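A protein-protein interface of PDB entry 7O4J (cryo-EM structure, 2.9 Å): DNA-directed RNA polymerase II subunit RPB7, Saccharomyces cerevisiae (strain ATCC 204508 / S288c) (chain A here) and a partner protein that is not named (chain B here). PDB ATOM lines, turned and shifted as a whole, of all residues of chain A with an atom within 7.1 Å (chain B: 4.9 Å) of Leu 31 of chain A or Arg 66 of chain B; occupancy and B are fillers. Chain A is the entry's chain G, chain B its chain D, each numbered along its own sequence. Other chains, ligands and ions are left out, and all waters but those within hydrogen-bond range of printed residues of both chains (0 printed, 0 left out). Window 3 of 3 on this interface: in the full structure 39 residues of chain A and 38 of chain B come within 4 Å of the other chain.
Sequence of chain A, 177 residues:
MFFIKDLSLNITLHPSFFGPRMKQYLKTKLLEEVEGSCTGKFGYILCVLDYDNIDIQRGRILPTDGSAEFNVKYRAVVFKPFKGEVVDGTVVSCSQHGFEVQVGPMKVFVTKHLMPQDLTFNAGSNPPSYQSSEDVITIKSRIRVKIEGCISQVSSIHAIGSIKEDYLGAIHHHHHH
Of the printed residues of chain B, Val 48 of chain A touches Arg 66 (3.0 Å). Printed residues of chain A within 4 Å of Leu 63 of chain B: Cys 47 (3.99 Å). Val 64 of chain B touches none of the printed residues of chain A. Arg 66 of chain B touches just these residues of chain A: Leu 31 (3.7 Å), Glu 35 (3.0 Å), Cys 47 (3.8 Å) and Val 48 (3.0 Å). The nearest residue of chain A that does not touch Arg 66 of chain B is Tyr 51 of chain A (4.1 Å).
Hydrophobic or aromatic side chains of chain A that line the printed part of chain B: Leu 31, Val 48, Leu 49 and Tyr 51. Along chain A the printed residues that touch a printed residue of chain B span positions 31 to 51. Among the printed residues, 7 pairs touch across the chains.
O of Leu 63 of chain B is in hydrogen-bond range of OG1 of Thr 133 of chain B (3.3 Å). The side-chain carboxylate (OE2) of Glu 35 of chain A sits at hydrogen-bond distance from the backbone NH (N) of Val 48 of chain A. The side-chain carboxylate (OE2) of Glu 35 of chain A lies close to the side-chain sulfur (SG) of Cys 47 of chain A (3.7 Å).
Among the printed residues, merely in contact across the chains: Tyr 51 of chain A with Phe 70 of chain B, Leu 31 of chain A with Arg 66 of chain B, Leu 49 of chain A with Ala 62 of chain B, Cys 47 of chain A with Arg 66 of chain B and Cys 47 of chain A with Leu 63 of chain B.
NH2 of Arg 66 of chain B is in salt-bridge range of OE2 of Glu 35 of chain A, 3.0 Å away. The guanidinium group (NH2) of Arg 66 of chain B sits at hydrogen-bond distance from the backbone carbonyl oxygen (O) of Val 48 of chain A, at 3.0 Å.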
ATOM      1  N   ILE A  11      -0.164  10.177 -10.731  1.00  0.00           N
ATOM      2  CA  ILE A  11       0.114   8.780 -11.039  1.00  0.00           C
ATOM      3  C   ILE A  11      -0.160   7.943  -9.800  1.00  0.00           C
ATOM      4  O   ILE A  11       0.067   8.377  -8.664  1.00  0.00           O
ATOM      5  CB  ILE A  11       1.563   8.583 -11.532  1.00  0.00           C
ATOM      6  CG1 ILE A  11       1.882   9.563 -12.662  1.00  0.00           C
ATOM      7  CG2 ILE A  11       1.773   7.149 -12.001  1.00  0.00           C
ATOM      8  CD1 ILE A  11       3.322   9.521 -13.116  1.00  0.00           C
ATOM      9  N   TYR A  25       9.840   3.022 -11.869  1.00  0.00           N
ATOM     10  CA  TYR A  25       8.494   2.627 -12.269  1.00  0.00           C
ATOM     11  C   TYR A  25       7.616   3.841 -12.537  1.00  0.00           C
ATOM     12  O   TYR A  25       6.812   3.829 -13.475  1.00  0.00           O
ATOM     13  CB  TYR A  25       7.866   1.742 -11.193  1.00  0.00           C
ATOM     14  CG  TYR A  25       8.594   0.434 -10.974  1.00  0.00           C
ATOM     15  CD1 TYR A  25       9.004  -0.346 -12.047  1.00  0.00           C
ATOM     16  CD2 TYR A  25       8.873  -0.022  -9.693  1.00  0.00           C
ATOM     17  CE1 TYR A  25       9.668  -1.541 -11.851  1.00  0.00           C
ATOM     18  CE2 TYR A  25       9.536  -1.215  -9.486  1.00  0.00           C
ATOM     19  CZ  TYR A  25       9.932  -1.971 -10.569  1.00  0.00           C
ATOM     20  OH  TYR A  25      10.594  -3.160 -10.369  1.00  0.00           O
ATOM     21  N   LEU A  26       7.750   4.894 -11.729  1.00  0.00           N
ATOM     22  CA  LEU A  26       6.980   6.109 -11.975  1.00  0.00           C
ATOM     23  C   LEU A  26       7.333   6.712 -13.329  1.00  0.00           C
ATOM     24  O   LEU A  26       6.448   7.170 -14.060  1.00  0.00           O
ATOM     25  CB  LEU A  26       7.225   7.123 -10.859  1.00  0.00           C
ATOM     26  CG  LEU A  26       6.441   6.915  -9.562  1.00  0.00           C
ATOM     27  CD1 LEU A  26       6.861   7.939  -8.524  1.00  0.00           C
ATOM     28  CD2 LEU A  26       4.943   6.991  -9.807  1.00  0.00           C
ATOM     29  N   LYS A  27       8.621   6.723 -13.678  1.00  0.00           N
ATOM     30  CA  LYS A  27       9.022   7.206 -14.994  1.00  0.00           C
ATOM     31  C   LYS A  27       8.425   6.341 -16.096  1.00  0.00           C
ATOM     32  O   LYS A  27       7.940   6.860 -17.109  1.00  0.00           O
ATOM     33  CB  LYS A  27      10.547   7.230 -15.104  1.00  0.00           C
ATOM     34  CG  LYS A  27      11.255   7.980 -13.986  1.00  0.00           C
ATOM     35  CD  LYS A  27      11.423   9.450 -14.319  1.00  0.00           C
ATOM     36  CE  LYS A  27      12.137  10.193 -13.203  1.00  0.00           C
ATOM     37  NZ  LYS A  27      13.497   9.646 -12.940  1.00  0.00           N
ATOM     38  N   THR A  28       8.449   5.020 -15.916  1.00  0.00           N
ATOM     39  CA  THR A  28       7.869   4.124 -16.910  1.00  0.00           C
ATOM     40  C   THR A  28       6.370   4.361 -17.044  1.00  0.00           C
ATOM     41  O   THR A  28       5.829   4.380 -18.156  1.00  0.00           O
ATOM     42  CB  THR A  28       8.153   2.670 -16.533  1.00  0.00           C
ATOM     43  OG1 THR A  28       9.564   2.426 -16.585  1.00  0.00           O
ATOM     44  CG2 THR A  28       7.441   1.718 -17.484  1.00  0.00           C
ATOM     45  N   LYS A  29       5.681   4.542 -15.916  1.00  0.00           N
ATOM     46  CA  LYS A  29       4.249   4.818 -15.965  1.00  0.00           C
ATOM     47  C   LYS A  29       3.967   6.126 -16.690  1.00  0.00           C
ATOM     48  O   LYS A  29       3.014   6.220 -17.472  1.00  0.00           O
ATOM     49  CB  LYS A  29       3.675   4.859 -14.549  1.00  0.00           C
ATOM     50  CG  LYS A  29       3.465   3.489 -13.920  1.00  0.00           C
ATOM     51  CD  LYS A  29       2.220   2.800 -14.463  1.00  0.00           C
ATOM     52  CE  LYS A  29       0.946   3.421 -13.909  1.00  0.00           C
ATOM     53  NZ  LYS A  29      -0.268   2.665 -14.321  1.00  0.00           N
ATOM     54  N   LEU A  30       4.786   7.151 -16.442  1.00  0.00           N
ATOM     55  CA  LEU A  30       4.586   8.434 -17.108  1.00  0.00           C
ATOM     56  C   LEU A  30       4.709   8.288 -18.619  1.00  0.00           C
ATOM     57  O   LEU A  30       3.883   8.812 -19.375  1.00  0.00           O
ATOM     58  CB  LEU A  30       5.595   9.455 -16.578  1.00  0.00           C
ATOM     59  CG  LEU A  30       5.377  10.913 -16.987  1.00  0.00           C
ATOM     60  CD1 LEU A  30       4.137  11.487 -16.323  1.00  0.00           C
ATOM     61  CD2 LEU A  30       6.600  11.747 -16.643  1.00  0.00           C
ATOM     62  N   LEU A  31       5.732   7.566 -19.081  1.00  0.00           N
ATOM     63  CA  LEU A  31       5.919   7.377 -20.513  1.00  0.00           C
ATOM     64  C   LEU A  31       4.867   6.461 -21.120  1.00  0.00           C
ATOM     65  O   LEU A  31       4.649   6.511 -22.334  1.00  0.00           O
ATOM     66  CB  LEU A  31       7.312   6.807 -20.794  1.00  0.00           C
ATOM     67  CG  LEU A  31       8.521   7.697 -20.495  1.00  0.00           C
ATOM     68  CD1 LEU A  31       9.773   7.093 -21.114  1.00  0.00           C
ATOM     69  CD2 LEU A  31       8.315   9.121 -20.990  1.00  0.00           C
ATOM     70  N   GLU A  32       4.216   5.625 -20.312  1.00  0.00           N
ATOM     71  CA  GLU A  32       3.211   4.699 -20.816  1.00  0.00           C
ATOM     72  C   GLU A  32       1.787   5.218 -20.672  1.00  0.00           C
ATOM     73  O   GLU A  32       0.894   4.720 -21.365  1.00  0.00           O
ATOM     74  CB  GLU A  32       3.323   3.352 -20.093  1.00  0.00           C
ATOM     75  CG  GLU A  32       4.299   2.381 -20.739  1.00  0.00           C
ATOM     76  CD  GLU A  32       3.973   0.933 -20.425  1.00  0.00           C
ATOM     77  OE1 GLU A  32       4.331   0.467 -19.324  1.00  0.00           O
ATOM     78  OE2 GLU A  32       3.359   0.263 -21.281  1.00  0.00           O
ATOM     79  N   GLU A  33       1.557   6.198 -19.800  1.00  0.00           N
ATOM     80  CA  GLU A  33       0.226   6.739 -19.573  1.00  0.00           C
ATOM     81  C   GLU A  33       0.044   8.147 -20.119  1.00  0.00           C
ATOM     82  O   GLU A  33      -1.098   8.607 -20.226  1.00  0.00           O
ATOM     83  CB  GLU A  33      -0.092   6.742 -18.069  1.00  0.00           C
ATOM     84  CG  GLU A  33      -1.581   6.759 -17.748  1.00  0.00           C
ATOM     85  CD  GLU A  33      -1.883   7.323 -16.371  1.00  0.00           C
ATOM     86  OE1 GLU A  33      -1.015   8.019 -15.802  1.00  0.00           O
ATOM     87  OE2 GLU A  33      -2.992   7.069 -15.855  1.00  0.00           O
ATOM     88  N   VAL A  34       1.127   8.841 -20.471  1.00  0.00           N
ATOM     89  CA  VAL A  34       1.071  10.216 -20.949  1.00  0.00           C
ATOM     90  C   VAL A  34       1.465  10.312 -22.418  1.00  0.00           C
ATOM     91  O   VAL A  34       0.737  10.892 -23.230  1.00  0.00           O
ATOM     92  CB  VAL A  34       1.959  11.143 -20.089  1.00  0.00           C
ATOM     93  CG1 VAL A  34       1.973  12.542 -20.661  1.00  0.00           C
ATOM     94  CG2 VAL A  34       1.469  11.158 -18.653  1.00  0.00           C
ATOM     95  N   GLU A  35       2.617   9.752 -22.778  1.00  0.00           N
ATOM     96  CA  GLU A  35       3.077   9.827 -24.158  1.00  0.00           C
ATOM     97  C   GLU A  35       2.068   9.164 -25.084  1.00  0.00           C
ATOM     98  O   GLU A  35       1.605   8.049 -24.825  1.00  0.00           O
ATOM     99  CB  GLU A  35       4.443   9.157 -24.298  1.00  0.00           C
ATOM    100  CG  GLU A  35       5.621  10.095 -24.097  1.00  0.00           C
ATOM    101  CD  GLU A  35       6.908   9.541 -24.673  1.00  0.00           C
ATOM    102  OE1 GLU A  35       7.050   8.302 -24.735  1.00  0.00           O
ATOM    103  OE2 GLU A  35       7.780  10.344 -25.066  1.00  0.00           O
ATOM    104  N   GLY A  36       1.727   9.855 -26.169  1.00  0.00           N
ATOM    105  CA  GLY A  36       0.754   9.360 -27.115  1.00  0.00           C
ATOM    106  C   GLY A  36      -0.687   9.541 -26.698  1.00  0.00           C
ATOM    107  O   GLY A  36      -1.586   9.235 -27.492  1.00  0.00           O
ATOM    108  N   LEU A  46       2.759  14.442 -26.903  1.00  0.00           N
ATOM    109  CA  LEU A  46       3.564  13.654 -27.830  1.00  0.00           C
ATOM    110  C   LEU A  46       4.823  13.097 -27.171  1.00  0.00           C
ATOM    111  O   LEU A  46       5.009  11.878 -27.104  1.00  0.00           O
ATOM    112  CB  LEU A  46       3.932  14.515 -29.042  1.00  0.00           C
ATOM    113  CG  LEU A  46       2.740  14.999 -29.866  1.00  0.00           C
ATOM    114  CD1 LEU A  46       3.179  16.068 -30.855  1.00  0.00           C
ATOM    115  CD2 LEU A  46       2.076  13.829 -30.574  1.00  0.00           C
ATOM    116  N   CYS A  47       5.693  13.977 -26.682  1.00  0.00           N
ATOM    117  CA  CYS A  47       6.986  13.584 -26.143  1.00  0.00           C
ATOM    118  C   CYS A  47       7.214  14.256 -24.800  1.00  0.00           C
ATOM    119  O   CYS A  47       6.787  15.394 -24.584  1.00  0.00           O
ATOM    120  CB  CYS A  47       8.118  13.953 -27.107  1.00  0.00           C
ATOM    121  SG  CYS A  47       9.609  12.950 -26.924  1.00  0.00           S
ATOM    122  N   VAL A  48       7.891  13.548 -23.903  1.00  0.00           N
ATOM    123  CA  VAL A  48       8.259  14.071 -22.593  1.00  0.00           C
ATOM    124  C   VAL A  48       9.712  14.517 -22.664  1.00  0.00           C
ATOM    125  O   VAL A  48      10.605  13.712 -22.956  1.00  0.00           O
ATOM    126  CB  VAL A  48       8.054  13.021 -21.490  1.00  0.00           C
ATOM    127  CG1 VAL A  48       8.475  13.578 -20.138  1.00  0.00           C
ATOM    128  CG2 VAL A  48       6.604  12.566 -21.452  1.00  0.00           C
ATOM    129  N   LEU A  49       9.951  15.797 -22.400  1.00  0.00           N
ATOM    130  CA  LEU A  49      11.291  16.357 -22.453  1.00  0.00           C
ATOM    131  C   LEU A  49      11.970  16.238 -21.095  1.00  0.00           C
ATOM    132  O   LEU A  49      11.325  16.305 -20.046  1.00  0.00           O
ATOM    133  CB  LEU A  49      11.247  17.822 -22.886  1.00  0.00           C
ATOM    134  CG  LEU A  49      10.550  18.101 -24.219  1.00  0.00           C
ATOM    135  CD1 LEU A  49      10.622  19.581 -24.554  1.00  0.00           C
ATOM    136  CD2 LEU A  49      11.155  17.268 -25.338  1.00  0.00           C
ATOM    137  N   ASP A  50      13.291  16.063 -21.126  1.00  0.00           N
ATOM    138  CA  ASP A  50      14.086  15.899 -19.912  1.00  0.00           C
ATOM    139  C   ASP A  50      13.590  14.700 -19.105  1.00  0.00           C
ATOM    140  O   ASP A  50      13.186  14.820 -17.947  1.00  0.00           O
ATOM    141  CB  ASP A  50      14.063  17.175 -19.068  1.00  0.00           C
ATOM    142  CG  ASP A  50      14.301  18.423 -19.894  1.00  0.00           C
ATOM    143  OD1 ASP A  50      15.021  18.337 -20.910  1.00  0.00           O
ATOM    144  OD2 ASP A  50      13.767  19.491 -19.526  1.00  0.00           O
ATOM    145  N   TYR A  51      13.631  13.524 -19.736  1.00  0.00           N
ATOM    146  CA  TYR A  51      13.138  12.315 -19.088  1.00  0.00           C
ATOM    147  C   TYR A  51      13.942  11.962 -17.844  1.00  0.00           C
ATOM    148  O   TYR A  51      13.475  11.169 -17.020  1.00  0.00           O
ATOM    149  CB  TYR A  51      13.161  11.151 -20.082  1.00  0.00           C
ATOM    150  CG  TYR A  51      13.051   9.785 -19.444  1.00  0.00           C
ATOM    151  CD1 TYR A  51      11.813   9.244 -19.129  1.00  0.00           C
ATOM    152  CD2 TYR A  51      14.185   9.036 -19.160  1.00  0.00           C
ATOM    153  CE1 TYR A  51      11.706   7.997 -18.546  1.00  0.00           C
ATOM    154  CE2 TYR A  51      14.087   7.787 -18.578  1.00  0.00           C
ATOM    155  CZ  TYR A  51      12.846   7.272 -18.273  1.00  0.00           C
ATOM    156  OH  TYR A  51      12.741   6.029 -17.693  1.00  0.00           O
ATOM    157  N   ILE A  54      12.421  14.470 -14.189  1.00  0.00           N
ATOM    158  CA  ILE A  54      11.041  14.653 -13.756  1.00  0.00           C
ATOM    159  C   ILE A  54      11.011  14.858 -12.249  1.00  0.00           C
ATOM    160  O   ILE A  54      11.748  14.206 -11.496  1.00  0.00           O
ATOM    161  CB  ILE A  54      10.169  13.456 -14.170  1.00  0.00           C
ATOM    162  CG1 ILE A  54      10.065  13.369 -15.693  1.00  0.00           C
ATOM    163  CG2 ILE A  54       8.782  13.570 -13.559  1.00  0.00           C
ATOM    164  CD1 ILE A  54      11.115  12.509 -16.326  1.00  0.00           C
ATOM    165  N   ALA B  62      15.168  14.618 -27.742  1.00  0.00           N
ATOM    166  CA  ALA B  62      14.864  13.940 -26.488  1.00  0.00           C
ATOM    167  C   ALA B  62      14.928  12.426 -26.632  1.00  0.00           C
ATOM    168  O   ALA B  62      15.321  11.734 -25.686  1.00  0.00           O
ATOM    169  CB  ALA B  62      13.482  14.358 -25.987  1.00  0.00           C
ATOM    170  N   LEU B  63      14.548  11.895 -27.796  1.00  0.00           N
ATOM    171  CA  LEU B  63      14.578  10.449 -27.991  1.00  0.00           C
ATOM    172  C   LEU B  63      15.999   9.908 -27.895  1.00  0.00           C
ATOM    173  O   LEU B  63      16.231   8.868 -27.269  1.00  0.00           O
ATOM    174  CB  LEU B  63      13.959  10.090 -29.341  1.00  0.00           C
ATOM    175  CG  LEU B  63      12.497  10.494 -29.549  1.00  0.00           C
ATOM    176  CD1 LEU B  63      12.040  10.120 -30.949  1.00  0.00           C
ATOM    177  CD2 LEU B  63      11.590   9.862 -28.504  1.00  0.00           C
ATOM    178  N   VAL B  64      16.963  10.597 -28.507  1.00  0.00           N
ATOM    179  CA  VAL B  64      18.347  10.141 -28.440  1.00  0.00           C
ATOM    180  C   VAL B  64      18.843  10.160 -27.000  1.00  0.00           C
ATOM    181  O   VAL B  64      19.519   9.227 -26.550  1.00  0.00           O
ATOM    182  CB  VAL B  64      19.246  10.986 -29.363  1.00  0.00           C
ATOM    183  CG1 VAL B  64      18.927  10.697 -30.823  1.00  0.00           C
ATOM    184  CG2 VAL B  64      19.105  12.477 -29.063  1.00  0.00           C
ATOM    185  N   GLU B  65      18.518  11.218 -26.254  1.00  0.00           N
ATOM    186  CA  GLU B  65      18.900  11.266 -24.847  1.00  0.00           C
ATOM    187  C   GLU B  65      18.234  10.142 -24.063  1.00  0.00           C
ATOM    188  O   GLU B  65      18.862   9.526 -23.194  1.00  0.00           O
ATOM    189  CB  GLU B  65      18.539  12.625 -24.250  1.00  0.00           C
ATOM    190  CG  GLU B  65      19.499  13.099 -23.172  1.00  0.00           C
ATOM    191  CD  GLU B  65      19.204  14.510 -22.704  1.00  0.00           C
ATOM    192  OE1 GLU B  65      19.628  14.868 -21.586  1.00  0.00           O
ATOM    193  OE2 GLU B  65      18.547  15.262 -23.455  1.00  0.00           O
ATOM    194  N   ARG B  66      16.962   9.864 -24.355  1.00  0.00           N
ATOM    195  CA  ARG B  66      16.282   8.754 -23.695  1.00  0.00           C
ATOM    196  C   ARG B  66      16.953   7.428 -24.026  1.00  0.00           C
ATOM    197  O   ARG B  66      17.121   6.571 -23.151  1.00  0.00           O
ATOM    198  CB  ARG B  66      14.809   8.729 -24.103  1.00  0.00           C
ATOM    199  CG  ARG B  66      13.948   7.805 -23.259  1.00  0.00           C
ATOM    200  CD  ARG B  66      12.500   7.829 -23.717  1.00  0.00           C
ATOM    201  NE  ARG B  66      11.862   9.112 -23.431  1.00  0.00           N
ATOM    202  CZ  ARG B  66      10.947   9.695 -24.201  1.00  0.00           C
ATOM    203  NH1 ARG B  66      10.535   9.117 -25.323  1.00  0.00           N
ATOM    204  NH2 ARG B  66      10.435  10.863 -23.844  1.00  0.00           N
ATOM    205  N   ARG B  67      17.346   7.239 -25.288  1.00  0.00           N
ATOM    206  CA  ARG B  67      18.078   6.032 -25.656  1.00  0.00           C
ATOM    207  C   ARG B  67      19.402   5.950 -24.907  1.00  0.00           C
ATOM    208  O   ARG B  67      19.803   4.871 -24.455  1.00  0.00           O
ATOM    209  CB  ARG B  67      18.315   5.999 -27.166  1.00  0.00           C
ATOM    210  CG  ARG B  67      19.299   4.929 -27.613  1.00  0.00           C
ATOM    211  CD  ARG B  67      19.259   4.727 -29.118  1.00  0.00           C
ATOM    212  NE  ARG B  67      19.653   5.933 -29.839  1.00  0.00           N
ATOM    213  CZ  ARG B  67      19.712   6.031 -31.164  1.00  0.00           C
ATOM    214  NH1 ARG B  67      19.401   4.991 -31.927  1.00  0.00           N
ATOM    215  NH2 ARG B  67      20.082   7.173 -31.727  1.00  0.00           N
ATOM    216  N   ARG B  68      20.095   7.082 -24.769  1.00  0.00           N
ATOM    217  CA  ARG B  68      21.348   7.097 -24.024  1.00  0.00           C
ATOM    218  C   ARG B  68      21.126   6.691 -22.572  1.00  0.00           C
ATOM    219  O   ARG B  68      21.955   5.988 -21.982  1.00  0.00           O
ATOM    220  CB  ARG B  68      21.983   8.486 -24.107  1.00  0.00           C
ATOM    221  CG  ARG B  68      23.305   8.622 -23.364  1.00  0.00           C
ATOM    222  CD  ARG B  68      23.760  10.073 -23.286  1.00  0.00           C
ATOM    223  NE  ARG B  68      23.537  10.794 -24.536  1.00  0.00           N
ATOM    224  CZ  ARG B  68      24.214  10.576 -25.660  1.00  0.00           C
ATOM    225  NH1 ARG B  68      25.169   9.657 -25.699  1.00  0.00           N
ATOM    226  NH2 ARG B  68      23.939  11.284 -26.747  1.00  0.00           N
ATOM    227  N   ALA B  69      20.013   7.125 -21.979  1.00  0.00           N
ATOM    228  CA  ALA B  69      19.743   6.812 -20.579  1.00  0.00           C
ATOM    229  C   ALA B  69      19.638   5.307 -20.363  1.00  0.00           C
ATOM    230  O   ALA B  69      20.273   4.747 -19.462  1.00  0.00           O
ATOM    231  CB  ALA B  69      18.460   7.513 -20.128  1.00  0.00           C
ATOM    232  N   PHE B  70      18.833   4.630 -21.186  1.00  0.00           N
ATOM    233  CA  PHE B  70      18.629   3.196 -21.000  1.00  0.00           C
ATOM    234  C   PHE B  70      19.907   2.412 -21.273  1.00  0.00           C
ATOM    235  O   PHE B  70      20.268   1.515 -20.502  1.00  0.00           O
ATOM    236  CB  PHE B  70      17.499   2.703 -21.906  1.00  0.00           C
ATOM    237  CG  PHE B  70      16.166   3.362 -21.650  1.00  0.00           C
ATOM    238  CD1 PHE B  70      15.958   4.146 -20.524  1.00  0.00           C
ATOM    239  CD2 PHE B  70      15.120   3.193 -22.541  1.00  0.00           C
ATOM    240  CE1 PHE B  70      14.733   4.745 -20.297  1.00  0.00           C
ATOM    241  CE2 PHE B  70      13.894   3.790 -22.318  1.00  0.00           C
ATOM    242  CZ  PHE B  70      13.700   4.566 -21.195  1.00  0.00           C
ATOM    243  N   THR B 133      13.037   3.325 -28.389  1.00  0.00           N
ATOM    244  CA  THR B 133      13.169   4.245 -27.266  1.00  0.00           C
ATOM    245  C   THR B 133      11.840   4.684 -26.662  1.00  0.00           C
ATOM    246  O   THR B 133      11.843   5.534 -25.767  1.00  0.00           O
ATOM    247  CB  THR B 133      13.954   5.485 -27.704  1.00  0.00           C
ATOM    248  OG1 THR B 133      14.391   6.211 -26.548  1.00  0.00           O
ATOM    249  CG2 THR B 133      13.087   6.386 -28.566  1.00  0.00           C
ATOM    250  N   THR B 134      10.715   4.140 -27.115  1.00  0.00           N
ATOM    251  CA  THR B 134       9.410   4.527 -26.602  1.00  0.00           C
ATOM    252  C   THR B 134       8.627   3.298 -26.163  1.00  0.00           C
ATOM    253  O   THR B 134       8.865   2.179 -26.627  1.00  0.00           O
ATOM    254  CB  THR B 134       8.602   5.310 -27.649  1.00  0.00           C
ATOM    255  OG1 THR B 134       8.111   4.413 -28.652  1.00  0.00           O
ATOM    256  CG2 THR B 134       9.461   6.391 -28.293  1.00  0.00           C
